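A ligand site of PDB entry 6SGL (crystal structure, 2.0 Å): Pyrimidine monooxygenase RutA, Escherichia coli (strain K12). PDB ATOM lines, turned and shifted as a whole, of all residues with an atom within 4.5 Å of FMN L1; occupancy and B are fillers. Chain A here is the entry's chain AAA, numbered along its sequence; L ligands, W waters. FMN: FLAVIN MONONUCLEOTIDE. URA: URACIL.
Residues that only touch FMN L1: Met 49 (3.1 Å), Thr 87 (3.3 Å), Leu 329 (3.4 Å), Phe 206 (3.5 Å), Gly 189 (3.5 Å), Phe 208 (3.6 Å), Gly 194 (3.6 Å), Phe 7 (3.6 Å), Trp 121 (3.9 Å) and Val 118 (3.9 Å). Hydrophobic or aromatic side chains within 4 Å of FMN L1: Phe 7, Met 49, Ile 50, Val 118, Trp 121, Tyr 142, Ala 188, Phe 206, Phe 208 and Leu 329. 16 residues have an atom within 4 Å of FMN L1: Phe 7, Met 49, Ile 50, Thr 87, Val 118, Trp 121, Arg 141, Tyr 142, Ala 188, Gly 189, Gln 190, Ser 191, Gly 194, Phe 206, Phe 208 and Leu 329. The nearest printed residue that does not touch FMN L1 is Asn 116 (4.02 Å).
N of Gln 190 lies within hydrogen-bond range of O2P of FMN L1. O4 of FMN L1 is in hydrogen-bond range of N of Ile 50, 2.8 Å away. The side-chain hydroxyl (OG) of Ser 191 is in hydrogen-bond range of an oxygen (O2P) of FMN L1, at 2.6 Å. An oxygen (O3') of FMN L1 sits at hydrogen-bond distance from the backbone carbonyl oxygen of Ala 188 (2.9 Å). The side-chain hydroxyl of Tyr 142 lies within hydrogen-bond range of an oxygen (O1P) of FMN L1, at 2.7 Å. O4 of URA L2 is in hydrogen-bond range of NE1 of Trp 121 (3.5 Å). The backbone NH (N) of Ser 191 is in hydrogen-bond range of an oxygen (O2P) of FMN L1 (3.0 Å). The backbone carbonyl oxygen of Ile 50 lies within hydrogen-bond range of a nitrogen (N3) of FMN L1 (3.3 Å). NH1 of Arg 141 is in salt-bridge range of O3P of FMN L1, at 2.5 Å. The side-chain amino group (NZ) of Lys 51 sits at hydrogen-bond distance from an oxygen (O4) of URA L2 (2.8 Å).
NH2 of Arg 141 sits at hydrogen-bond distance from OG1 of Thr 119, at 2.9 Å. The side-chain amide oxygen (OE1) of Gln 190 sits close to the backbone carbonyl oxygen (O) of Phe 206 (3.1 Å). OG1 of Thr 87 lies within hydrogen-bond range of ND2 of Asn 116, at 3.3 Å. The backbone NH (N) of Gly 194 lies within hydrogen-bond range of the side-chain hydroxyl (OG) of Ser 191 (3.0 Å). NE2 of Gln 190 sits close to N of Phe 208 (3.4 Å).
Water W1 lies within hydrogen-bond range of the backbone NH of Thr 119, the side-chain hydroxyl of Tyr 142 and an oxygen (O2') of FMN L1.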
ATOM      1  N   PHE A   7     -18.479 -15.481  31.400  1.00  0.00           N
ATOM      2  CA  PHE A   7     -18.041 -14.346  30.608  1.00  0.00           C
ATOM      3  C   PHE A   7     -16.658 -13.941  31.123  1.00  0.00           C
ATOM      4  O   PHE A   7     -16.553 -13.398  32.223  1.00  0.00           O
ATOM      5  CB  PHE A   7     -19.061 -13.220  30.772  1.00  0.00           C
ATOM      6  CG  PHE A   7     -19.241 -12.276  29.607  1.00  0.00           C
ATOM      7  CD1 PHE A   7     -18.747 -12.577  28.343  1.00  0.00           C
ATOM      8  CD2 PHE A   7     -19.908 -11.086  29.759  1.00  0.00           C
ATOM      9  CE1 PHE A   7     -18.916 -11.707  27.263  1.00  0.00           C
ATOM     10  CE2 PHE A   7     -20.121 -10.233  28.683  1.00  0.00           C
ATOM     11  CZ  PHE A   7     -19.614 -10.529  27.434  1.00  0.00           C
ATOM     12  N   LEU A  47     -17.120 -17.538  27.155  1.00  0.00           N
ATOM     13  CA  LEU A  47     -17.141 -16.597  26.039  1.00  0.00           C
ATOM     14  C   LEU A  47     -16.269 -15.401  26.400  1.00  0.00           C
ATOM     15  O   LEU A  47     -16.402 -14.823  27.486  1.00  0.00           O
ATOM     16  CB  LEU A  47     -18.591 -16.132  25.885  1.00  0.00           C
ATOM     17  CG  LEU A  47     -18.807 -14.848  25.090  1.00  0.00           C
ATOM     18  CD1 LEU A  47     -18.439 -15.028  23.622  1.00  0.00           C
ATOM     19  CD2 LEU A  47     -20.301 -14.465  25.174  1.00  0.00           C
ATOM     20  N   MET A  49     -15.787 -11.425  25.114  1.00  0.00           N
ATOM     21  CA  MET A  49     -16.076 -10.292  24.255  1.00  0.00           C
ATOM     22  C   MET A  49     -14.827  -9.813  23.503  1.00  0.00           C
ATOM     23  O   MET A  49     -13.743 -10.371  23.650  1.00  0.00           O
ATOM     24  CB  MET A  49     -16.653  -9.158  25.103  1.00  0.00           C
ATOM     25  CG  MET A  49     -15.703  -8.641  26.198  1.00  0.00           C
ATOM     26  SD  MET A  49     -16.322  -7.012  26.792  1.00  0.00           S
ATOM     27  CE  MET A  49     -14.912  -6.547  27.798  1.00  0.00           C
ATOM     28  N   ILE A  50     -15.008  -8.809  22.642  1.00  0.00           N
ATOM     29  CA  ILE A  50     -13.896  -8.061  22.069  1.00  0.00           C
ATOM     30  C   ILE A  50     -14.193  -6.579  22.368  1.00  0.00           C
ATOM     31  O   ILE A  50     -15.337  -6.145  22.277  1.00  0.00           O
ATOM     32  CB  ILE A  50     -13.695  -8.364  20.558  1.00  0.00           C
ATOM     33  CG1 ILE A  50     -12.449  -7.693  19.956  1.00  0.00           C
ATOM     34  CG2 ILE A  50     -14.956  -8.003  19.768  1.00  0.00           C
ATOM     35  CD1 ILE A  50     -11.079  -8.205  20.455  1.00  0.00           C
ATOM     36  N   LYS A  51     -13.187  -5.841  22.828  1.00  0.00           N
ATOM     37  CA  LYS A  51     -13.392  -4.432  23.179  1.00  0.00           C
ATOM     38  C   LYS A  51     -12.135  -3.609  22.868  1.00  0.00           C
ATOM     39  O   LYS A  51     -11.161  -3.610  23.635  1.00  0.00           O
ATOM     40  CB  LYS A  51     -13.846  -4.305  24.633  1.00  0.00           C
ATOM     41  CG  LYS A  51     -14.058  -2.884  25.170  1.00  0.00           C
ATOM     42  CD  LYS A  51     -15.145  -2.039  24.534  1.00  0.00           C
ATOM     43  CE  LYS A  51     -16.546  -2.508  24.888  1.00  0.00           C
ATOM     44  NZ  LYS A  51     -16.999  -3.550  23.929  1.00  0.00           N
ATOM     45  N   THR A  87     -15.435 -13.737  20.107  1.00  0.00           N
ATOM     46  CA  THR A  87     -16.213 -12.731  19.423  1.00  0.00           C
ATOM     47  C   THR A  87     -15.430 -12.177  18.236  1.00  0.00           C
ATOM     48  O   THR A  87     -14.282 -11.785  18.412  1.00  0.00           O
ATOM     49  CB  THR A  87     -16.527 -11.558  20.365  1.00  0.00           C
ATOM     50  OG1 THR A  87     -17.204 -12.252  21.388  1.00  0.00           O
ATOM     51  CG2 THR A  87     -17.514 -10.558  19.809  1.00  0.00           C
ATOM     52  N   ASN A 116     -19.031 -15.754  18.200  1.00  0.00           N
ATOM     53  CA  ASN A 116     -20.055 -14.771  18.516  1.00  0.00           C
ATOM     54  C   ASN A 116     -19.850 -13.622  17.528  1.00  0.00           C
ATOM     55  O   ASN A 116     -18.753 -13.076  17.460  1.00  0.00           O
ATOM     56  CB  ASN A 116     -19.970 -14.335  19.982  1.00  0.00           C
ATOM     57  CG  ASN A 116     -20.966 -13.256  20.352  1.00  0.00           C
ATOM     58  OD1 ASN A 116     -22.098 -13.239  19.883  1.00  0.00           O
ATOM     59  ND2 ASN A 116     -20.541 -12.353  21.230  1.00  0.00           N
ATOM     60  N   VAL A 118     -20.699  -9.952  16.110  1.00  0.00           N
ATOM     61  CA  VAL A 118     -21.241  -8.664  16.521  1.00  0.00           C
ATOM     62  C   VAL A 118     -21.016  -7.667  15.381  1.00  0.00           C
ATOM     63  O   VAL A 118     -20.020  -7.727  14.640  1.00  0.00           O
ATOM     64  CB  VAL A 118     -20.600  -8.152  17.836  1.00  0.00           C
ATOM     65  CG1 VAL A 118     -20.861  -9.086  19.016  1.00  0.00           C
ATOM     66  CG2 VAL A 118     -19.124  -7.877  17.660  1.00  0.00           C
ATOM     67  N   THR A 119     -21.959  -6.730  15.285  1.00  0.00           N
ATOM     68  CA  THR A 119     -21.920  -5.686  14.275  1.00  0.00           C
ATOM     69  C   THR A 119     -20.959  -4.576  14.708  1.00  0.00           C
ATOM     70  O   THR A 119     -20.307  -3.952  13.874  1.00  0.00           O
ATOM     71  CB  THR A 119     -23.307  -5.069  14.054  1.00  0.00           C
ATOM     72  OG1 THR A 119     -23.676  -4.519  15.313  1.00  0.00           O
ATOM     73  CG2 THR A 119     -24.359  -6.058  13.580  1.00  0.00           C
ATOM     74  N   GLY A 120     -20.912  -4.330  16.021  1.00  0.00           N
ATOM     75  CA  GLY A 120     -20.175  -3.211  16.589  1.00  0.00           C
ATOM     76  C   GLY A 120     -21.092  -2.014  16.761  1.00  0.00           C
ATOM     77  O   GLY A 120     -21.672  -1.519  15.797  1.00  0.00           O
ATOM     78  N   TRP A 121     -21.216  -1.550  18.018  1.00  0.00           N
ATOM     79  CA  TRP A 121     -22.055  -0.409  18.334  1.00  0.00           C
ATOM     80  C   TRP A 121     -21.194   0.854  18.512  1.00  0.00           C
ATOM     81  O   TRP A 121     -21.543   1.918  18.000  1.00  0.00           O
ATOM     82  CB  TRP A 121     -22.963  -0.707  19.537  1.00  0.00           C
ATOM     83  CG  TRP A 121     -22.264  -0.928  20.848  1.00  0.00           C
ATOM     84  CD1 TRP A 121     -21.866  -2.116  21.384  1.00  0.00           C
ATOM     85  CD2 TRP A 121     -21.876   0.088  21.806  1.00  0.00           C
ATOM     86  NE1 TRP A 121     -21.260  -1.923  22.600  1.00  0.00           N
ATOM     87  CE2 TRP A 121     -21.249  -0.581  22.884  1.00  0.00           C
ATOM     88  CE3 TRP A 121     -21.992   1.483  21.853  1.00  0.00           C
ATOM     89  CZ2 TRP A 121     -20.755   0.099  23.998  1.00  0.00           C
ATOM     90  CZ3 TRP A 121     -21.496   2.158  22.953  1.00  0.00           C
ATOM     91  CH2 TRP A 121     -20.883   1.470  24.008  1.00  0.00           C
ATOM     92  N   ARG A 141     -26.265  -2.270   9.430  1.00  0.00           N
ATOM     93  CA  ARG A 141     -25.287  -3.199   9.971  1.00  0.00           C
ATOM     94  C   ARG A 141     -25.704  -4.663   9.812  1.00  0.00           C
ATOM     95  O   ARG A 141     -24.841  -5.540   9.695  1.00  0.00           O
ATOM     96  CB  ARG A 141     -25.008  -2.878  11.436  1.00  0.00           C
ATOM     97  CG  ARG A 141     -26.230  -2.984  12.333  1.00  0.00           C
ATOM     98  CD  ARG A 141     -25.877  -2.085  13.476  1.00  0.00           C
ATOM     99  NE  ARG A 141     -26.992  -1.882  14.381  1.00  0.00           N
ATOM    100  CZ  ARG A 141     -27.145  -2.509  15.539  1.00  0.00           C
ATOM    101  NH1 ARG A 141     -28.201  -2.223  16.290  1.00  0.00           N
ATOM    102  NH2 ARG A 141     -26.254  -3.398  15.951  1.00  0.00           N
ATOM    103  N   TYR A 142     -27.017  -4.934   9.821  1.00  0.00           N
ATOM    104  CA  TYR A 142     -27.579  -6.287   9.745  1.00  0.00           C
ATOM    105  C   TYR A 142     -27.591  -6.793   8.305  1.00  0.00           C
ATOM    106  O   TYR A 142     -27.501  -8.001   8.078  1.00  0.00           O
ATOM    107  CB  TYR A 142     -28.860  -6.415  10.578  1.00  0.00           C
ATOM    108  CG  TYR A 142     -28.599  -6.595  12.059  1.00  0.00           C
ATOM    109  CD1 TYR A 142     -27.950  -7.729  12.512  1.00  0.00           C
ATOM    110  CD2 TYR A 142     -28.914  -5.618  12.997  1.00  0.00           C
ATOM    111  CE1 TYR A 142     -27.628  -7.908  13.850  1.00  0.00           C
ATOM    112  CE2 TYR A 142     -28.598  -5.770  14.347  1.00  0.00           C
ATOM    113  CZ  TYR A 142     -27.956  -6.936  14.774  1.00  0.00           C
ATOM    114  OH  TYR A 142     -27.635  -7.177  16.093  1.00  0.00           O
ATOM    115  N   ALA A 188     -25.835 -11.556  19.554  1.00  0.00           N
ATOM    116  CA  ALA A 188     -26.311 -10.856  20.736  1.00  0.00           C
ATOM    117  C   ALA A 188     -27.255  -9.726  20.320  1.00  0.00           C
ATOM    118  O   ALA A 188     -27.244  -8.655  20.894  1.00  0.00           O
ATOM    119  CB  ALA A 188     -25.108 -10.350  21.513  1.00  0.00           C
ATOM    120  N   GLY A 189     -28.132  -9.995  19.342  1.00  0.00           N
ATOM    121  CA  GLY A 189     -29.063  -8.975  18.896  1.00  0.00           C
ATOM    122  C   GLY A 189     -30.227  -8.786  19.865  1.00  0.00           C
ATOM    123  O   GLY A 189     -30.829  -9.764  20.321  1.00  0.00           O
ATOM    124  N   GLN A 190     -30.528  -7.513  20.182  1.00  0.00           N
ATOM    125  CA  GLN A 190     -31.607  -7.142  21.081  1.00  0.00           C
ATOM    126  C   GLN A 190     -32.725  -6.496  20.273  1.00  0.00           C
ATOM    127  O   GLN A 190     -33.907  -6.589  20.607  1.00  0.00           O
ATOM    128  CB  GLN A 190     -31.149  -6.123  22.142  1.00  0.00           C
ATOM    129  CG  GLN A 190     -30.063  -6.594  23.105  1.00  0.00           C
ATOM    130  CD  GLN A 190     -30.337  -7.906  23.789  1.00  0.00           C
ATOM    131  OE1 GLN A 190     -30.051  -8.976  23.249  1.00  0.00           O
ATOM    132  NE2 GLN A 190     -30.847  -7.844  25.021  1.00  0.00           N
ATOM    133  N   SER A 191     -32.357  -5.792  19.211  1.00  0.00           N
ATOM    134  CA  SER A 191     -33.298  -5.106  18.352  1.00  0.00           C
ATOM    135  C   SER A 191     -34.108  -6.112  17.517  1.00  0.00           C
ATOM    136  O   SER A 191     -33.852  -7.326  17.517  1.00  0.00           O
ATOM    137  CB  SER A 191     -32.562  -4.163  17.443  1.00  0.00           C
ATOM    138  OG  SER A 191     -31.782  -4.888  16.521  1.00  0.00           O
ATOM    139  N   GLY A 194     -31.884  -7.425  14.849  1.00  0.00           N
ATOM    140  CA  GLY A 194     -30.897  -8.269  15.493  1.00  0.00           C
ATOM    141  C   GLY A 194     -31.437  -9.675  15.740  1.00  0.00           C
ATOM    142  O   GLY A 194     -30.775 -10.651  15.422  1.00  0.00           O
ATOM    143  N   PHE A 206     -27.712 -14.204  22.838  1.00  0.00           N
ATOM    144  CA  PHE A 206     -27.420 -13.609  24.128  1.00  0.00           C
ATOM    145  C   PHE A 206     -28.281 -12.371  24.332  1.00  0.00           C
ATOM    146  O   PHE A 206     -28.291 -11.486  23.478  1.00  0.00           O
ATOM    147  CB  PHE A 206     -25.963 -13.143  24.200  1.00  0.00           C
ATOM    148  CG  PHE A 206     -25.039 -14.310  24.392  1.00  0.00           C
ATOM    149  CD1 PHE A 206     -25.077 -15.048  25.566  1.00  0.00           C
ATOM    150  CD2 PHE A 206     -24.209 -14.740  23.380  1.00  0.00           C
ATOM    151  CE1 PHE A 206     -24.291 -16.181  25.734  1.00  0.00           C
ATOM    152  CE2 PHE A 206     -23.395 -15.859  23.560  1.00  0.00           C
ATOM    153  CZ  PHE A 206     -23.453 -16.590  24.722  1.00  0.00           C
ATOM    154  N   CYS A 207     -28.927 -12.306  25.493  1.00  0.00           N
ATOM    155  CA  CYS A 207     -29.620 -11.090  25.886  1.00  0.00           C
ATOM    156  C   CYS A 207     -29.265 -10.698  27.325  1.00  0.00           C
ATOM    157  O   CYS A 207     -28.745 -11.526  28.049  1.00  0.00           O
ATOM    158  CB  CYS A 207     -31.122 -11.281  25.734  1.00  0.00           C
ATOM    159  SG  CYS A 207     -31.811 -12.521  26.854  1.00  0.00           S
ATOM    160  N   PHE A 208     -29.572  -9.450  27.714  1.00  0.00           N
ATOM    161  CA  PHE A 208     -29.286  -8.904  29.039  1.00  0.00           C
ATOM    162  C   PHE A 208     -30.308  -9.373  30.069  1.00  0.00           C
ATOM    163  O   PHE A 208     -31.499  -9.319  29.811  1.00  0.00           O
ATOM    164  CB  PHE A 208     -29.265  -7.373  28.968  1.00  0.00           C
ATOM    165  CG  PHE A 208     -28.180  -6.829  28.079  1.00  0.00           C
ATOM    166  CD1 PHE A 208     -26.858  -6.825  28.505  1.00  0.00           C
ATOM    167  CD2 PHE A 208     -28.460  -6.392  26.797  1.00  0.00           C
ATOM    168  CE1 PHE A 208     -25.852  -6.359  27.675  1.00  0.00           C
ATOM    169  CE2 PHE A 208     -27.453  -5.917  25.963  1.00  0.00           C
ATOM    170  CZ  PHE A 208     -26.154  -5.889  26.416  1.00  0.00           C
ATOM    171  N   LEU A 329     -25.279 -16.602  31.145  1.00  0.00           N
ATOM    172  CA  LEU A 329     -23.879 -16.241  31.082  1.00  0.00           C
ATOM    173  C   LEU A 329     -23.568 -15.362  32.300  1.00  0.00           C
ATOM    174  O   LEU A 329     -24.165 -14.300  32.471  1.00  0.00           O
ATOM    175  CB  LEU A 329     -23.750 -15.440  29.788  1.00  0.00           C
ATOM    176  CG  LEU A 329     -22.398 -14.793  29.518  1.00  0.00           C
ATOM    177  CD1 LEU A 329     -21.317 -15.835  29.253  1.00  0.00           C
ATOM    178  CD2 LEU A 329     -22.515 -13.796  28.388  1.00  0.00           C
HETATM  179  N1  FMN L   1     -20.689  -5.794  21.482  1.00  0.00           N
HETATM  180  C2  FMN L   1     -19.422  -5.655  21.012  1.00  0.00           C
HETATM  181  O2  FMN L   1     -19.147  -4.671  20.295  1.00  0.00           O
HETATM  182  N3  FMN L   1     -18.443  -6.554  21.287  1.00  0.00           N
HETATM  183  C4  FMN L   1     -18.692  -7.633  22.067  1.00  0.00           C
HETATM  184  O4  FMN L   1     -17.788  -8.455  22.275  1.00  0.00           O
HETATM  185  C4A FMN L   1     -20.063  -7.891  22.619  1.00  0.00           C
HETATM  186  N5  FMN L   1     -20.402  -8.959  23.382  1.00  0.00           N
HETATM  187  C5A FMN L   1     -21.657  -9.096  23.883  1.00  0.00           C
HETATM  188  C6  FMN L   1     -21.981 -10.212  24.690  1.00  0.00           C
HETATM  189  C7  FMN L   1     -23.247 -10.363  25.235  1.00  0.00           C
HETATM  190  C7M FMN L   1     -23.493 -11.572  26.070  1.00  0.00           C
HETATM  191  C8  FMN L   1     -24.332  -9.338  24.931  1.00  0.00           C
HETATM  192  C8M FMN L   1     -25.749  -9.441  25.431  1.00  0.00           C
HETATM  193  C9  FMN L   1     -24.024  -8.225  24.140  1.00  0.00           C
HETATM  194  C9A FMN L   1     -22.723  -8.073  23.604  1.00  0.00           C
HETATM  195  N10 FMN L   1     -22.391  -6.966  22.779  1.00  0.00           N
HETATM  196  C10 FMN L   1     -21.073  -6.858  22.271  1.00  0.00           C
HETATM  197  C1' FMN L   1     -23.349  -5.910  22.416  1.00  0.00           C
HETATM  198  C2' FMN L   1     -24.493  -6.530  21.637  1.00  0.00           C
HETATM  199  O2' FMN L   1     -24.005  -6.892  20.329  1.00  0.00           O
HETATM  200  C3' FMN L   1     -25.741  -5.608  21.788  1.00  0.00           C
HETATM  201  O3' FMN L   1     -26.834  -6.250  22.464  1.00  0.00           O
HETATM  202  C4' FMN L   1     -26.265  -5.144  20.471  1.00  0.00           C
HETATM  203  O4' FMN L   1     -25.211  -4.443  19.799  1.00  0.00           O
HETATM  204  C5' FMN L   1     -27.587  -4.369  20.672  1.00  0.00           C
HETATM  205  O5' FMN L   1     -28.544  -5.111  19.870  1.00  0.00           O
HETATM  206  P   FMN L   1     -28.683  -4.745  18.312  1.00  0.00           P
HETATM  207  O1P FMN L   1     -27.326  -4.959  17.664  1.00  0.00           O
HETATM  208  O2P FMN L   1     -29.702  -5.725  17.790  1.00  0.00           O
HETATM  209  O3P FMN L   1     -29.079  -3.307  18.408  1.00  0.00           O
HETATM  210  N1  URA L   2     -21.099  -5.847  27.949  1.00  0.00           N
HETATM  211  C2  URA L   2     -21.783  -4.832  27.329  1.00  0.00           C
HETATM  212  O2  URA L   2     -22.833  -4.365  27.759  1.00  0.00           O
HETATM  213  N3  URA L   2     -21.210  -4.365  26.156  1.00  0.00           N
HETATM  214  C4  URA L   2     -20.034  -4.828  25.579  1.00  0.00           C
HETATM  215  O4  URA L   2     -19.627  -4.311  24.544  1.00  0.00           O
HETATM  216  C5  URA L   2     -19.391  -5.891  26.309  1.00  0.00           C
HETATM  217  C6  URA L   2     -19.932  -6.362  27.454  1.00  0.00           C
HETATM  218  O   HOH W   1     -24.503  -7.562  17.085  1.00  0.00           O
